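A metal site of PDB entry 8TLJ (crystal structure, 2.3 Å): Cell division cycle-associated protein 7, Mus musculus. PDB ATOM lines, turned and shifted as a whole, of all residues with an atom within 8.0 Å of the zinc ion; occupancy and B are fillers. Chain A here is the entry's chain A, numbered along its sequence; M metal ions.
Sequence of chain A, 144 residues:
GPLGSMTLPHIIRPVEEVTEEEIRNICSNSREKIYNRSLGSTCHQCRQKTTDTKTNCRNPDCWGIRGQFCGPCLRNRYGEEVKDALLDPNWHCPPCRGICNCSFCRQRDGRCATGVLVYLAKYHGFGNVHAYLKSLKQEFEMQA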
ATOM      1  N   SER A  30      30.808  -7.863  25.621  1.00  0.00           N
ATOM      2  CA  SER A  30      29.529  -7.294  26.038  1.00  0.00           C
ATOM      3  C   SER A  30      28.396  -8.310  26.028  1.00  0.00           C
ATOM      4  O   SER A  30      27.418  -8.132  26.767  1.00  0.00           O
ATOM      5  CB  SER A  30      29.166  -6.097  25.151  1.00  0.00           C
ATOM      6  OG  SER A  30      29.133  -6.465  23.783  1.00  0.00           O
ATOM      7  N   LYS A  33      27.603  -9.999  29.592  1.00  0.00           N
ATOM      8  CA  LYS A  33      27.223  -9.187  30.736  1.00  0.00           C
ATOM      9  C   LYS A  33      26.013  -9.785  31.454  1.00  0.00           C
ATOM     10  O   LYS A  33      25.179 -10.479  30.858  1.00  0.00           O
ATOM     11  CB  LYS A  33      26.908  -7.757  30.291  1.00  0.00           C
ATOM     12  CG  LYS A  33      28.124  -6.974  29.823  1.00  0.00           C
ATOM     13  CD  LYS A  33      27.740  -5.556  29.428  1.00  0.00           C
ATOM     14  CE  LYS A  33      28.978  -4.738  29.067  1.00  0.00           C
ATOM     15  NZ  LYS A  33      28.615  -3.335  28.746  1.00  0.00           N
ATOM     16  N   THR A  42      25.679   1.200  35.738  1.00  0.00           N
ATOM     17  CA  THR A  42      25.471   1.629  34.357  1.00  0.00           C
ATOM     18  C   THR A  42      26.769   2.121  33.735  1.00  0.00           C
ATOM     19  O   THR A  42      27.480   2.944  34.336  1.00  0.00           O
ATOM     20  CB  THR A  42      24.411   2.741  34.300  1.00  0.00           C
ATOM     21  OG1 THR A  42      23.192   2.273  34.898  1.00  0.00           O
ATOM     22  CG2 THR A  42      24.143   3.156  32.858  1.00  0.00           C
ATOM     23  N   CYS A  43      27.088   1.621  32.548  1.00  0.00           N
ATOM     24  CA  CYS A  43      28.164   2.188  31.748  1.00  0.00           C
ATOM     25  C   CYS A  43      27.645   3.421  31.025  1.00  0.00           C
ATOM     26  O   CYS A  43      26.586   3.378  30.398  1.00  0.00           O
ATOM     27  CB  CYS A  43      28.690   1.160  30.749  1.00  0.00           C
ATOM     28  SG  CYS A  43      29.850   1.842  29.511  1.00  0.00           S
ATOM     29  N   HIS A  44      28.377   4.529  31.125  1.00  0.00           N
ATOM     30  CA  HIS A  44      27.942   5.761  30.475  1.00  0.00           C
ATOM     31  C   HIS A  44      27.858   5.595  28.960  1.00  0.00           C
ATOM     32  O   HIS A  44      26.947   6.142  28.321  1.00  0.00           O
ATOM     33  CB  HIS A  44      28.886   6.909  30.819  1.00  0.00           C
ATOM     34  CG  HIS A  44      28.627   8.161  30.030  1.00  0.00           C
ATOM     35  ND1 HIS A  44      27.508   8.946  30.237  1.00  0.00           N
ATOM     36  CD2 HIS A  44      29.320   8.738  29.027  1.00  0.00           C
ATOM     37  CE1 HIS A  44      27.544   9.969  29.392  1.00  0.00           C
ATOM     38  NE2 HIS A  44      28.629   9.861  28.655  1.00  0.00           N
ATOM     39  N   GLN A  45      28.777   4.832  28.376  1.00  0.00           N
ATOM     40  CA  GLN A  45      28.853   4.731  26.911  1.00  0.00           C
ATOM     41  C   GLN A  45      27.676   3.938  26.354  1.00  0.00           C
ATOM     42  O   GLN A  45      26.885   4.465  25.559  1.00  0.00           O
ATOM     43  CB  GLN A  45      30.185   4.088  26.501  1.00  0.00           C
ATOM     44  CG  GLN A  45      30.449   4.108  25.000  1.00  0.00           C
ATOM     45  CD  GLN A  45      31.024   5.433  24.522  1.00  0.00           C
ATOM     46  OE1 GLN A  45      31.510   6.235  25.318  1.00  0.00           O
ATOM     47  NE2 GLN A  45      30.961   5.671  23.217  1.00  0.00           N
ATOM     48  N   CYS A  46      27.541   2.673  26.742  1.00  0.00           N
ATOM     49  CA  CYS A  46      26.492   1.814  26.210  1.00  0.00           C
ATOM     50  C   CYS A  46      25.198   1.879  27.001  1.00  0.00           C
ATOM     51  O   CYS A  46      24.193   1.311  26.557  1.00  0.00           O
ATOM     52  CB  CYS A  46      26.988   0.363  26.139  1.00  0.00           C
ATOM     53  SG  CYS A  46      27.396  -0.381  27.738  1.00  0.00           S
ATOM     54  N   ARG A  47      25.198   2.552  28.149  1.00  0.00           N
ATOM     55  CA  ARG A  47      23.983   2.783  28.937  1.00  0.00           C
ATOM     56  C   ARG A  47      23.286   1.479  29.311  1.00  0.00           C
ATOM     57  O   ARG A  47      22.057   1.386  29.332  1.00  0.00           O
ATOM     58  CB  ARG A  47      23.026   3.728  28.198  1.00  0.00           C
ATOM     59  CG  ARG A  47      23.701   5.045  27.787  1.00  0.00           C
ATOM     60  CD  ARG A  47      22.700   6.081  27.314  1.00  0.00           C
ATOM     61  NE  ARG A  47      22.178   5.798  25.983  1.00  0.00           N
ATOM     62  CZ  ARG A  47      22.712   6.251  24.855  1.00  0.00           C
ATOM     63  NH1 ARG A  47      23.798   7.017  24.869  1.00  0.00           N
ATOM     64  NH2 ARG A  47      22.145   5.942  23.702  1.00  0.00           N
ATOM     65  N   GLN A  48      24.083   0.459  29.620  1.00  0.00           N
ATOM     66  CA  GLN A  48      23.588  -0.812  30.139  1.00  0.00           C
ATOM     67  C   GLN A  48      23.974  -0.921  31.611  1.00  0.00           C
ATOM     68  O   GLN A  48      25.108  -0.618  31.985  1.00  0.00           O
ATOM     69  CB  GLN A  48      24.158  -2.005  29.361  1.00  0.00           C
ATOM     70  CG  GLN A  48      23.985  -1.921  27.848  1.00  0.00           C
ATOM     71  CD  GLN A  48      22.533  -1.784  27.418  1.00  0.00           C
ATOM     72  OE1 GLN A  48      21.779  -2.756  27.410  1.00  0.00           O
ATOM     73  NE2 GLN A  48      22.132  -0.566  27.070  1.00  0.00           N
ATOM     74  N   THR A  50      24.771  -3.299  34.385  1.00  0.00           N
ATOM     75  CA  THR A  50      25.207  -4.682  34.521  1.00  0.00           C
ATOM     76  C   THR A  50      26.164  -4.796  35.697  1.00  0.00           C
ATOM     77  O   THR A  50      26.640  -3.786  36.248  1.00  0.00           O
ATOM     78  CB  THR A  50      25.871  -5.190  33.240  1.00  0.00           C
ATOM     79  OG1 THR A  50      27.017  -4.374  32.929  1.00  0.00           O
ATOM     80  CG2 THR A  50      24.897  -5.163  32.067  1.00  0.00           C
ATOM     81  N   ASP A  52      29.224  -6.206  35.844  1.00  0.00           N
ATOM     82  CA  ASP A  52      30.665  -6.249  35.619  1.00  0.00           C
ATOM     83  C   ASP A  52      31.335  -4.986  36.181  1.00  0.00           C
ATOM     84  O   ASP A  52      30.711  -3.927  36.308  1.00  0.00           O
ATOM     85  CB  ASP A  52      30.991  -6.404  34.141  1.00  0.00           C
ATOM     86  CG  ASP A  52      30.113  -5.539  33.257  1.00  0.00           C
ATOM     87  OD1 ASP A  52      28.903  -5.840  33.153  1.00  0.00           O
ATOM     88  OD2 ASP A  52      30.626  -4.570  32.664  1.00  0.00           O
ATOM     89  N   LYS A  54      33.366  -1.650  36.537  1.00  0.00           N
ATOM     90  CA  LYS A  54      33.440  -0.475  35.693  1.00  0.00           C
ATOM     91  C   LYS A  54      34.438   0.519  36.285  1.00  0.00           C
ATOM     92  O   LYS A  54      34.858   0.392  37.436  1.00  0.00           O
ATOM     93  CB  LYS A  54      32.056   0.178  35.526  1.00  0.00           C
ATOM     94  CG  LYS A  54      30.949  -0.847  35.285  1.00  0.00           C
ATOM     95  CD  LYS A  54      29.912  -0.350  34.303  1.00  0.00           C
ATOM     96  CE  LYS A  54      29.046  -1.494  33.820  1.00  0.00           C
ATOM     97  NZ  LYS A  54      28.483  -2.293  34.953  1.00  0.00           N
ATOM     98  N   GLN A  68      31.596   6.127  34.723  1.00  0.00           N
ATOM     99  CA  GLN A  68      31.572   4.675  34.827  1.00  0.00           C
ATOM    100  C   GLN A  68      31.519   4.073  33.425  1.00  0.00           C
ATOM    101  O   GLN A  68      30.571   4.314  32.684  1.00  0.00           O
ATOM    102  CB  GLN A  68      30.373   4.207  35.659  1.00  0.00           C
ATOM    103  CG  GLN A  68      30.328   4.828  37.052  1.00  0.00           C
ATOM    104  CD  GLN A  68      29.089   4.449  37.840  1.00  0.00           C
ATOM    105  OE1 GLN A  68      28.239   3.698  37.364  1.00  0.00           O
ATOM    106  NE2 GLN A  68      28.982   4.971  39.057  1.00  0.00           N
ATOM    107  N   PHE A  69      32.542   3.288  33.086  1.00  0.00           N
ATOM    108  CA  PHE A  69      32.657   2.674  31.773  1.00  0.00           C
ATOM    109  C   PHE A  69      32.968   1.189  31.906  1.00  0.00           C
ATOM    110  O   PHE A  69      33.793   0.788  32.740  1.00  0.00           O
ATOM    111  CB  PHE A  69      33.747   3.355  30.927  1.00  0.00           C
ATOM    112  CG  PHE A  69      33.376   4.722  30.442  1.00  0.00           C
ATOM    113  CD1 PHE A  69      33.442   5.823  31.284  1.00  0.00           C
ATOM    114  CD2 PHE A  69      32.958   4.907  29.134  1.00  0.00           C
ATOM    115  CE1 PHE A  69      33.098   7.081  30.838  1.00  0.00           C
ATOM    116  CE2 PHE A  69      32.605   6.166  28.683  1.00  0.00           C
ATOM    117  CZ  PHE A  69      32.676   7.253  29.535  1.00  0.00           C
ATOM    118  N   CYS A  70      32.304   0.386  31.088  1.00  0.00           N
ATOM    119  CA  CYS A  70      32.545  -1.055  31.061  1.00  0.00           C
ATOM    120  C   CYS A  70      33.798  -1.376  30.263  1.00  0.00           C
ATOM    121  O   CYS A  70      34.332  -0.544  29.524  1.00  0.00           O
ATOM    122  CB  CYS A  70      31.335  -1.787  30.479  1.00  0.00           C
ATOM    123  SG  CYS A  70      31.101  -1.550  28.690  1.00  0.00           S
ATOM    124  N   GLY A  71      34.262  -2.613  30.414  1.00  0.00           N
ATOM    125  CA  GLY A  71      35.471  -3.076  29.759  1.00  0.00           C
ATOM    126  C   GLY A  71      35.442  -2.929  28.245  1.00  0.00           C
ATOM    127  O   GLY A  71      36.323  -2.293  27.658  1.00  0.00           O
ATOM    128  N   PRO A  72      34.448  -3.534  27.585  1.00  0.00           N
ATOM    129  CA  PRO A  72      34.380  -3.410  26.125  1.00  0.00           C
ATOM    130  C   PRO A  72      34.288  -1.971  25.635  1.00  0.00           C
ATOM    131  O   PRO A  72      34.921  -1.619  24.625  1.00  0.00           O
ATOM    132  CB  PRO A  72      33.115  -4.206  25.763  1.00  0.00           C
ATOM    133  CG  PRO A  72      32.997  -5.209  26.855  1.00  0.00           C
ATOM    134  CD  PRO A  72      33.476  -4.523  28.102  1.00  0.00           C
ATOM    135  N   CYS A  73      33.534  -1.118  26.323  1.00  0.00           N
ATOM    136  CA  CYS A  73      33.367   0.254  25.856  1.00  0.00           C
ATOM    137  C   CYS A  73      34.663   1.055  25.983  1.00  0.00           C
ATOM    138  O   CYS A  73      34.986   1.855  25.095  1.00  0.00           O
ATOM    139  CB  CYS A  73      32.227   0.940  26.615  1.00  0.00           C
ATOM    140  SG  CYS A  73      30.588   0.555  25.977  1.00  0.00           S
ATOM    141  N   LEU A  74      35.398   0.863  27.072  1.00  0.00           N
ATOM    142  CA  LEU A  74      36.598   1.672  27.277  1.00  0.00           C
ATOM    143  C   LEU A  74      37.682   1.349  26.254  1.00  0.00           C
ATOM    144  O   LEU A  74      38.347   2.254  25.743  1.00  0.00           O
ATOM    145  CB  LEU A  74      37.122   1.492  28.701  1.00  0.00           C
ATOM    146  CG  LEU A  74      38.060   2.608  29.157  1.00  0.00           C
ATOM    147  CD1 LEU A  74      37.319   3.939  29.224  1.00  0.00           C
ATOM    148  CD2 LEU A  74      38.696   2.285  30.498  1.00  0.00           C
ATOM    149  N   ARG A  77      36.209   2.152  22.408  1.00  0.00           N
ATOM    150  CA  ARG A  77      35.924   3.549  22.114  1.00  0.00           C
ATOM    151  C   ARG A  77      37.039   4.492  22.547  1.00  0.00           C
ATOM    152  O   ARG A  77      37.042   5.649  22.111  1.00  0.00           O
ATOM    153  CB  ARG A  77      34.611   3.973  22.770  1.00  0.00           C
ATOM    154  CG  ARG A  77      33.444   3.042  22.500  1.00  0.00           C
ATOM    155  CD  ARG A  77      32.979   3.117  21.048  1.00  0.00           C
ATOM    156  NE  ARG A  77      32.474   4.448  20.725  1.00  0.00           N
ATOM    157  CZ  ARG A  77      31.706   4.711  19.668  1.00  0.00           C
ATOM    158  NH1 ARG A  77      31.326   3.759  18.834  1.00  0.00           N
ATOM    159  NH2 ARG A  77      31.304   5.961  19.463  1.00  0.00           N
HETATM  160 ZN    ZN M   1      29.625   0.084  27.999  1.00  0.00          ZN
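SG of Cys 73 is bound to the zinc ion, at 2.3 Å. SG of Cys 46 is bound to the zinc ion (2.3 Å). SG of Cys 70 binds the zinc ion, 2.3 Å away. SG of Cys 43 binds the zinc ion (2.3 Å). The zinc ion has four donor atoms within binding distance.
NZ of Lys 33 touches the zinc ion, 3.6 Å away. Of the 20 residues printed, 5 come within 4 Å of the zinc ion. Along chain A the residues within 4 Å of the zinc ion span positions 33 to 73. The nearest printed residue that does not touch the zinc ion is Gln 45 (4.3 Å).
The side-chain sulfur (SG) of Cys 46 sits close to the side-chain amino group (NZ) of Lys 33 (3.4 Å). The backbone carbonyl oxygen (O) of Cys 46 sits at hydrogen-bond distance from the side-chain amide nitrogen (NE2) of Gln 48 (2.8 Å). NZ of Lys 33 lies close to SG of Cys 70. N of Gln 45 sits close to SG of Cys 43. The backbone NH (N) of Cys 43 lies within hydrogen-bond range of the backbone carbonyl oxygen (O) of Gln 48 (3.0 Å).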
